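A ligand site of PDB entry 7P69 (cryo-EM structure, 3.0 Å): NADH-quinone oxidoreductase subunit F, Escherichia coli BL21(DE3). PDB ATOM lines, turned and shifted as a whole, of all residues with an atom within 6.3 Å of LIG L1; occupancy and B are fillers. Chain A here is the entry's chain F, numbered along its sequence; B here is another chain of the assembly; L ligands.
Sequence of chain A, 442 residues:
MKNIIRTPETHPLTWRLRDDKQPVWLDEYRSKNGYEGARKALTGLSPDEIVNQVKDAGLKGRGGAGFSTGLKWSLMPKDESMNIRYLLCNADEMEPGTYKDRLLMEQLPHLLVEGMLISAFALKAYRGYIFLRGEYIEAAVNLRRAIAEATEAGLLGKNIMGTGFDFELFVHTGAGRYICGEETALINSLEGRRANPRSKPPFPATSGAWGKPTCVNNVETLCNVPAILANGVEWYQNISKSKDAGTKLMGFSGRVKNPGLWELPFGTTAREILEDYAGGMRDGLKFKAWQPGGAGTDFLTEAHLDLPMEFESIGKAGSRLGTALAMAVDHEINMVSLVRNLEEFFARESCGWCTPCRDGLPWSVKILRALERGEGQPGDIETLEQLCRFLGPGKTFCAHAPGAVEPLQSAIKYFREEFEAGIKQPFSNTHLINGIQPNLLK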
ATOM      1  N   ILE A 179     -30.816   2.212  -4.834  1.00  0.00           N
ATOM      2  CA  ILE A 179     -31.352   2.222  -3.479  1.00  0.00           C
ATOM      3  C   ILE A 179     -32.386   3.328  -3.280  1.00  0.00           C
ATOM      4  O   ILE A 179     -33.178   3.253  -2.337  1.00  0.00           O
ATOM      5  CB  ILE A 179     -30.190   2.339  -2.476  1.00  0.00           C
ATOM      6  CG1 ILE A 179     -30.600   1.854  -1.091  1.00  0.00           C
ATOM      7  CG2 ILE A 179     -29.653   3.751  -2.410  1.00  0.00           C
ATOM      8  CD1 ILE A 179     -31.307   0.516  -1.099  1.00  0.00           C
ATOM      9  N   ASN A 196     -29.755   6.833   2.161  1.00  0.00           N
ATOM     10  CA  ASN A 196     -29.746   5.717   3.088  1.00  0.00           C
ATOM     11  C   ASN A 196     -31.178   5.410   3.516  1.00  0.00           C
ATOM     12  O   ASN A 196     -31.938   6.327   3.826  1.00  0.00           O
ATOM     13  CB  ASN A 196     -28.896   6.030   4.302  1.00  0.00           C
ATOM     14  CG  ASN A 196     -27.451   6.244   3.961  1.00  0.00           C
ATOM     15  OD1 ASN A 196     -26.928   7.346   4.119  1.00  0.00           O
ATOM     16  ND2 ASN A 196     -26.792   5.195   3.509  1.00  0.00           N
ATOM     17  N   PRO A 197     -31.561   4.136   3.547  1.00  0.00           N
ATOM     18  CA  PRO A 197     -32.866   3.784   4.087  1.00  0.00           C
ATOM     19  C   PRO A 197     -32.940   4.035   5.584  1.00  0.00           C
ATOM     20  O   PRO A 197     -31.928   4.250   6.264  1.00  0.00           O
ATOM     21  CB  PRO A 197     -32.996   2.287   3.767  1.00  0.00           C
ATOM     22  CG  PRO A 197     -31.615   1.839   3.502  1.00  0.00           C
ATOM     23  CD  PRO A 197     -30.873   2.989   2.940  1.00  0.00           C
ATOM     24  N   GLU A 349     -24.401  -0.997  -6.202  1.00  0.00           N
ATOM     25  CA  GLU A 349     -25.572  -0.205  -5.880  1.00  0.00           C
ATOM     26  C   GLU A 349     -25.884  -0.198  -4.398  1.00  0.00           C
ATOM     27  O   GLU A 349     -26.945   0.294  -3.994  1.00  0.00           O
ATOM     28  CB  GLU A 349     -26.777  -0.677  -6.680  1.00  0.00           C
ATOM     29  CG  GLU A 349     -26.717  -0.307  -8.142  1.00  0.00           C
ATOM     30  CD  GLU A 349     -26.607   1.189  -8.365  1.00  0.00           C
ATOM     31  OE1 GLU A 349     -27.294   1.954  -7.664  1.00  0.00           O
ATOM     32  OE2 GLU A 349     -25.831   1.603  -9.250  1.00  0.00           O
ATOM     33  N   SER A 350     -24.989  -0.737  -3.582  1.00  0.00           N
ATOM     34  CA  SER A 350     -25.121  -0.640  -2.129  1.00  0.00           C
ATOM     35  C   SER A 350     -25.020   0.812  -1.698  1.00  0.00           C
ATOM     36  O   SER A 350     -24.407   1.643  -2.372  1.00  0.00           O
ATOM     37  CB  SER A 350     -24.029  -1.467  -1.468  1.00  0.00           C
ATOM     38  OG  SER A 350     -24.060  -1.345  -0.057  1.00  0.00           O
ATOM     39  N   CYS A 351     -25.667   1.142  -0.593  1.00  0.00           N
ATOM     40  CA  CYS A 351     -25.591   2.504  -0.095  1.00  0.00           C
ATOM     41  C   CYS A 351     -24.456   2.686   0.904  1.00  0.00           C
ATOM     42  O   CYS A 351     -24.110   3.831   1.211  1.00  0.00           O
ATOM     43  CB  CYS A 351     -26.927   2.914   0.533  1.00  0.00           C
ATOM     44  SG  CYS A 351     -27.180   2.396   2.232  1.00  0.00           S
ATOM     45  N   GLY A 352     -23.868   1.605   1.391  1.00  0.00           N
ATOM     46  CA  GLY A 352     -22.741   1.692   2.291  1.00  0.00           C
ATOM     47  C   GLY A 352     -23.076   1.858   3.748  1.00  0.00           C
ATOM     48  O   GLY A 352     -22.164   2.059   4.551  1.00  0.00           O
ATOM     49  N   TRP A 353     -24.353   1.789   4.114  1.00  0.00           N
ATOM     50  CA  TRP A 353     -24.734   2.029   5.500  1.00  0.00           C
ATOM     51  C   TRP A 353     -24.335   0.873   6.407  1.00  0.00           C
ATOM     52  O   TRP A 353     -23.759   1.079   7.475  1.00  0.00           O
ATOM     53  CB  TRP A 353     -26.233   2.289   5.597  1.00  0.00           C
ATOM     54  CG  TRP A 353     -26.751   2.453   6.969  1.00  0.00           C
ATOM     55  CD1 TRP A 353     -27.496   1.569   7.665  1.00  0.00           C
ATOM     56  CD2 TRP A 353     -26.545   3.578   7.829  1.00  0.00           C
ATOM     57  NE1 TRP A 353     -27.790   2.066   8.907  1.00  0.00           N
ATOM     58  CE2 TRP A 353     -27.212   3.291   9.039  1.00  0.00           C
ATOM     59  CE3 TRP A 353     -25.861   4.782   7.704  1.00  0.00           C
ATOM     60  CZ2 TRP A 353     -27.214   4.175  10.100  1.00  0.00           C
ATOM     61  CZ3 TRP A 353     -25.876   5.660   8.763  1.00  0.00           C
ATOM     62  CH2 TRP A 353     -26.540   5.359   9.953  1.00  0.00           C
ATOM     63  N   CYS A 354     -24.602  -0.361   5.988  1.00  0.00           N
ATOM     64  CA  CYS A 354     -24.489  -1.475   6.908  1.00  0.00           C
ATOM     65  C   CYS A 354     -23.481  -2.502   6.428  1.00  0.00           C
ATOM     66  O   CYS A 354     -23.281  -2.705   5.221  1.00  0.00           O
ATOM     67  CB  CYS A 354     -25.875  -2.105   7.178  1.00  0.00           C
ATOM     68  SG  CYS A 354     -26.576  -3.224   5.993  1.00  0.00           S
ATOM     69  N   THR A 355     -22.829  -3.142   7.398  1.00  0.00           N
ATOM     70  CA  THR A 355     -21.653  -3.980   7.145  1.00  0.00           C
ATOM     71  C   THR A 355     -21.879  -5.181   6.232  1.00  0.00           C
ATOM     72  O   THR A 355     -21.057  -5.381   5.329  1.00  0.00           O
ATOM     73  CB  THR A 355     -21.048  -4.427   8.480  1.00  0.00           C
ATOM     74  OG1 THR A 355     -20.741  -3.283   9.276  1.00  0.00           O
ATOM     75  CG2 THR A 355     -19.783  -5.221   8.268  1.00  0.00           C
ATOM     76  N   PRO A 356     -22.922  -6.030   6.409  1.00  0.00           N
ATOM     77  CA  PRO A 356     -22.978  -7.253   5.588  1.00  0.00           C
ATOM     78  C   PRO A 356     -23.106  -6.981   4.102  1.00  0.00           C
ATOM     79  O   PRO A 356     -22.355  -7.579   3.325  1.00  0.00           O
ATOM     80  CB  PRO A 356     -24.208  -7.970   6.136  1.00  0.00           C
ATOM     81  CG  PRO A 356     -24.370  -7.465   7.475  1.00  0.00           C
ATOM     82  CD  PRO A 356     -24.036  -6.034   7.358  1.00  0.00           C
ATOM     83  N   CYS A 357     -23.965  -6.056   3.687  1.00  0.00           N
ATOM     84  CA  CYS A 357     -24.058  -5.706   2.281  1.00  0.00           C
ATOM     85  C   CYS A 357     -22.753  -5.067   1.790  1.00  0.00           C
ATOM     86  O   CYS A 357     -22.104  -5.616   0.886  1.00  0.00           O
ATOM     87  CB  CYS A 357     -25.253  -4.775   2.095  1.00  0.00           C
ATOM     88  SG  CYS A 357     -25.578  -3.968   0.536  1.00  0.00           S
ATOM     89  N   ARG A 358     -22.283  -4.033   2.489  1.00  0.00           N
ATOM     90  CA  ARG A 358     -21.140  -3.229   2.058  1.00  0.00           C
ATOM     91  C   ARG A 358     -19.851  -4.027   1.958  1.00  0.00           C
ATOM     92  O   ARG A 358     -19.051  -3.800   1.037  1.00  0.00           O
ATOM     93  CB  ARG A 358     -20.949  -2.048   3.023  1.00  0.00           C
ATOM     94  CG  ARG A 358     -19.625  -1.314   2.896  1.00  0.00           C
ATOM     95  CD  ARG A 358     -19.433  -0.218   3.912  1.00  0.00           C
ATOM     96  NE  ARG A 358     -19.053  -0.759   5.204  1.00  0.00           N
ATOM     97  CZ  ARG A 358     -19.837  -0.787   6.269  1.00  0.00           C
ATOM     98  NH1 ARG A 358     -21.041  -0.253   6.251  1.00  0.00           N
ATOM     99  NH2 ARG A 358     -19.393  -1.364   7.384  1.00  0.00           N
ATOM    100  N   LEU A 361     -21.166  -8.321  -0.046  1.00  0.00           N
ATOM    101  CA  LEU A 361     -21.392  -8.379  -1.484  1.00  0.00           C
ATOM    102  C   LEU A 361     -20.107  -8.276  -2.301  1.00  0.00           C
ATOM    103  O   LEU A 361     -19.988  -9.038  -3.274  1.00  0.00           O
ATOM    104  CB  LEU A 361     -22.421  -7.330  -1.901  1.00  0.00           C
ATOM    105  CG  LEU A 361     -23.853  -7.631  -1.452  1.00  0.00           C
ATOM    106  CD1 LEU A 361     -24.777  -6.558  -1.963  1.00  0.00           C
ATOM    107  CD2 LEU A 361     -24.273  -8.991  -1.963  1.00  0.00           C
ATOM    108  N   THR A 396     -29.362  -7.530   7.671  1.00  0.00           N
ATOM    109  CA  THR A 396     -28.941  -6.254   7.113  1.00  0.00           C
ATOM    110  C   THR A 396     -29.958  -5.178   7.463  1.00  0.00           C
ATOM    111  O   THR A 396     -31.055  -5.448   7.938  1.00  0.00           O
ATOM    112  CB  THR A 396     -28.773  -6.353   5.604  1.00  0.00           C
ATOM    113  OG1 THR A 396     -30.000  -6.788   5.008  1.00  0.00           O
ATOM    114  CG2 THR A 396     -27.691  -7.335   5.272  1.00  0.00           C
ATOM    115  N   PHE A 397     -29.569  -3.930   7.206  1.00  0.00           N
ATOM    116  CA  PHE A 397     -30.392  -2.800   7.612  1.00  0.00           C
ATOM    117  C   PHE A 397     -31.632  -2.670   6.732  1.00  0.00           C
ATOM    118  O   PHE A 397     -32.718  -2.357   7.233  1.00  0.00           O
ATOM    119  CB  PHE A 397     -29.567  -1.518   7.582  1.00  0.00           C
ATOM    120  CG  PHE A 397     -30.253  -0.353   8.217  1.00  0.00           C
ATOM    121  CD1 PHE A 397     -30.262  -0.210   9.594  1.00  0.00           C
ATOM    122  CD2 PHE A 397     -30.866   0.608   7.443  1.00  0.00           C
ATOM    123  CE1 PHE A 397     -30.893   0.873  10.176  1.00  0.00           C
ATOM    124  CE2 PHE A 397     -31.486   1.683   8.023  1.00  0.00           C
ATOM    125  CZ  PHE A 397     -31.496   1.813   9.394  1.00  0.00           C
ATOM    126  N   CYS A 398     -31.488  -2.896   5.431  1.00  0.00           N
ATOM    127  CA  CYS A 398     -32.659  -2.872   4.551  1.00  0.00           C
ATOM    128  C   CYS A 398     -32.726  -4.135   3.719  1.00  0.00           C
ATOM    129  O   CYS A 398     -31.919  -5.055   3.900  1.00  0.00           O
ATOM    130  CB  CYS A 398     -32.642  -1.635   3.664  1.00  0.00           C
ATOM    131  SG  CYS A 398     -31.779  -1.805   2.096  1.00  0.00           S
ATOM    132  N   ALA A 399     -33.674  -4.186   2.791  1.00  0.00           N
ATOM    133  CA  ALA A 399     -33.958  -5.400   2.028  1.00  0.00           C
ATOM    134  C   ALA A 399     -33.180  -5.494   0.727  1.00  0.00           C
ATOM    135  O   ALA A 399     -33.491  -6.351  -0.103  1.00  0.00           O
ATOM    136  CB  ALA A 399     -35.460  -5.479   1.732  1.00  0.00           C
ATOM    137  N   HIS A 400     -32.177  -4.632   0.529  1.00  0.00           N
ATOM    138  CA  HIS A 400     -31.372  -4.703  -0.685  1.00  0.00           C
ATOM    139  C   HIS A 400     -30.519  -5.964  -0.724  1.00  0.00           C
ATOM    140  O   HIS A 400     -30.446  -6.639  -1.762  1.00  0.00           O
ATOM    141  CB  HIS A 400     -30.496  -3.458  -0.797  1.00  0.00           C
ATOM    142  CG  HIS A 400     -29.431  -3.551  -1.834  1.00  0.00           C
ATOM    143  ND1 HIS A 400     -29.674  -3.312  -3.169  1.00  0.00           N
ATOM    144  CD2 HIS A 400     -28.112  -3.837  -1.748  1.00  0.00           C
ATOM    145  CE1 HIS A 400     -28.557  -3.455  -3.854  1.00  0.00           C
ATOM    146  NE2 HIS A 400     -27.591  -3.772  -3.009  1.00  0.00           N
ATOM    147  N   ALA A 401     -29.893  -6.322   0.386  1.00  0.00           N
ATOM    148  CA  ALA A 401     -29.016  -7.483   0.434  1.00  0.00           C
ATOM    149  C   ALA A 401     -29.733  -8.842   0.441  1.00  0.00           C
ATOM    150  O   ALA A 401     -29.184  -9.782  -0.152  1.00  0.00           O
ATOM    151  CB  ALA A 401     -28.082  -7.383   1.641  1.00  0.00           C
ATOM    152  N   PRO A 402     -30.898  -9.026   1.084  1.00  0.00           N
ATOM    153  CA  PRO A 402     -31.650 -10.273   0.823  1.00  0.00           C
ATOM    154  C   PRO A 402     -32.041 -10.451  -0.629  1.00  0.00           C
ATOM    155  O   PRO A 402     -31.954 -11.567  -1.172  1.00  0.00           O
ATOM    156  CB  PRO A 402     -32.873 -10.129   1.737  1.00  0.00           C
ATOM    157  CG  PRO A 402     -32.402  -9.313   2.845  1.00  0.00           C
ATOM    158  CD  PRO A 402     -31.469  -8.320   2.254  1.00  0.00           C
ATOM    159  N   HIS B 175     -21.221   2.612  -2.079  1.00  0.00           N
ATOM    160  CA  HIS B 175     -21.311   1.209  -1.701  1.00  0.00           C
ATOM    161  C   HIS B 175     -20.280   0.653  -0.729  1.00  0.00           C
ATOM    162  O   HIS B 175     -20.658   0.184   0.349  1.00  0.00           O
ATOM    163  CB  HIS B 175     -21.176   0.438  -3.011  1.00  0.00           C
ATOM    164  CG  HIS B 175     -20.310   1.141  -4.007  1.00  0.00           C
ATOM    165  ND1 HIS B 175     -18.933   1.053  -3.997  1.00  0.00           N
ATOM    166  CD2 HIS B 175     -20.619   1.966  -5.041  1.00  0.00           C
ATOM    167  CE1 HIS B 175     -18.430   1.784  -4.970  1.00  0.00           C
ATOM    168  NE2 HIS B 175     -19.442   2.346  -5.623  1.00  0.00           N
HETATM  169 FE1  LIG L   1     -27.382  -2.111   4.107  1.00  0.00          FE
HETATM  170 FE2  LIG L   1     -26.983  -2.422   1.552  1.00  0.00          FE
HETATM  171 FE3  LIG L   1     -29.473  -1.662   2.393  1.00  0.00          FE
HETATM  172 FE4  LIG L   1     -27.514   0.102   2.447  1.00  0.00          FE
HETATM  173  S1  LIG L   1     -28.352  -0.869   0.540  1.00  0.00           S
HETATM  174  S2  LIG L   1     -28.901  -0.393   4.218  1.00  0.00           S
HETATM  175  S3  LIG L   1     -25.654  -1.150   2.942  1.00  0.00           S
HETATM  176  S4  LIG L   1     -28.452  -3.669   2.812  1.00  0.00           S
HETATM  177  N1  LG2 L   2     -40.552   0.183  -5.405  1.00  0.00           N
HETATM  178  C1  LG2 L   2     -40.854   0.841  -6.574  1.00  0.00           C
HETATM  179  O1  LG2 L   2     -42.015   1.104  -6.833  1.00  0.00           O
HETATM  180  N2  LG2 L   2     -39.851   1.190  -7.441  1.00  0.00           N
HETATM  181  C2  LG2 L   2     -38.546   0.880  -7.139  1.00  0.00           C
HETATM  182  O2  LG2 L   2     -37.650   1.185  -7.903  1.00  0.00           O
HETATM  183  C3  LG2 L   2     -38.249   0.224  -5.957  1.00  0.00           C
HETATM  184  N3  LG2 L   2     -36.944  -0.085  -5.655  1.00  0.00           N
HETATM  185  C4  LG2 L   2     -36.650  -0.732  -4.476  1.00  0.00           C
HETATM  186  C5  LG2 L   2     -35.328  -1.032  -4.200  1.00  0.00           C
HETATM  187  C6  LG2 L   2     -35.002  -1.679  -3.026  1.00  0.00           C
HETATM  188  C7  LG2 L   2     -33.566  -1.990  -2.745  1.00  0.00           C
HETATM  189  C8  LG2 L   2     -36.002  -2.044  -2.141  1.00  0.00           C
HETATM  190  C9  LG2 L   2     -35.660  -2.758  -0.869  1.00  0.00           C
HETATM  191  C10 LG2 L   2     -37.328  -1.748  -2.424  1.00  0.00           C
HETATM  192  C11 LG2 L   2     -37.670  -1.084  -3.598  1.00  0.00           C
HETATM  193  N4  LG2 L   2     -38.974  -0.775  -3.900  1.00  0.00           N
HETATM  194  C12 LG2 L   2     -39.260  -0.126  -5.085  1.00  0.00           C
HETATM  195  C13 LG2 L   2     -40.110  -1.136  -2.980  1.00  0.00           C
HETATM  196  C14 LG2 L   2     -40.443   0.048  -2.066  1.00  0.00           C
HETATM  197  O3  LG2 L   2     -39.712  -0.084  -0.873  1.00  0.00           O
HETATM  198  C15 LG2 L   2     -41.927   0.148  -1.729  1.00  0.00           C
HETATM  199  O4  LG2 L   2     -42.398  -1.093  -1.258  1.00  0.00           O
HETATM  200  C16 LG2 L   2     -42.747   0.586  -2.932  1.00  0.00           C
HETATM  201  O5  LG2 L   2     -42.082   1.638  -3.590  1.00  0.00           O
HETATM  202  C17 LG2 L   2     -44.165   1.029  -2.595  1.00  0.00           C
HETATM  203  O6  LG2 L   2     -44.931  -0.074  -2.189  1.00  0.00           O
HETATM  204  P1  LG2 L   2     -46.319  -0.429  -2.920  1.00  0.00           P
HETATM  205  O7  LG2 L   2     -46.049  -1.586  -3.851  1.00  0.00           O
HETATM  206  O8  LG2 L   2     -47.351  -0.825  -1.905  1.00  0.00           O
HETATM  207  O9  LG2 L   2     -46.813   0.730  -3.729  1.00  0.00           O
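SG of Cys 351 sits close to N of Trp 353 (3.4 Å). SG of Cys 351 sits close to ND2 of Asn 196. The backbone carbonyl oxygen (O) of Cys 398 is in hydrogen-bond range of the side-chain hydroxyl (OG1) of Thr 396, 2.8 Å away. The backbone carbonyl oxygen (O) of Cys 354 sits close to the guanidinium group (NH1) of Arg 358 (3.5 Å). The side-chain hydroxyl of Ser 350 lies within hydrogen-bond range of the backbone NH of Gly 352 (3.3 Å). O of Ser 350 lies close to N of His 175 of chain B, at 3.3 Å. O of Trp 353 sits at hydrogen-bond distance from NH1 of Arg 358 (3.3 Å). The backbone carbonyl oxygen (O) of Gly 352 is in hydrogen-bond range of the guanidinium group (NH1) of Arg 358, at 3.1 Å.
Residues that only touch LIG L1: Ile 179 (3.7 Å), Pro 197 (3.6 Å), Thr 396 (3.9 Å), Phe 397 (3.6 Å), His 400 (3.6 Å) and Ala 401 (3.9 Å). Hydrophobic or aromatic side chains within 4 Å of LIG L1: Ile 179, Pro 197, Phe 397, His 400 and Ala 401. Within 4 Å of LIG L1: Ile 179, Pro 197, Ser 350, Cys 351, Gly 352, Trp 353, Cys 354, Cys 357, Thr 396, Phe 397, Cys 398, His 400 and Ala 401. The nearest printed residue that does not touch LIG L1 is Arg 358 (4.5 Å).
The side-chain sulfur (SG) of Cys 357 binds an iron atom (FE2) of LIG L1 (2.3 Å). N of Cys 351 lies close to S1 of LIG L1, at 3.5 Å. The side-chain sulfur of Cys 351 binds an iron atom (FE4) of LIG L1 (2.3 Å). A sulfur (S2) of LIG L1 sits close to the backbone NH of Cys 398, at 3.8 Å. The side-chain sulfur (SG) of Cys 398 is bound to an iron atom (FE3) of LIG L1 (2.3 Å). S3 of LIG L1 lies close to N of Cys 354, 3.3 Å away. An iron atom (FE1) of LIG L1 is bound by the side-chain sulfur (SG) of Cys 354. S3 of LIG L1 sits close to OG of Ser 350 (3.4 Å). The backbone NH of Trp 353 sits close to a sulfur (S3) of LIG L1, 3.4 Å away. A sulfur (S3) of LIG L1 sits close to the backbone NH (N) of Gly 352 (3.6 Å).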
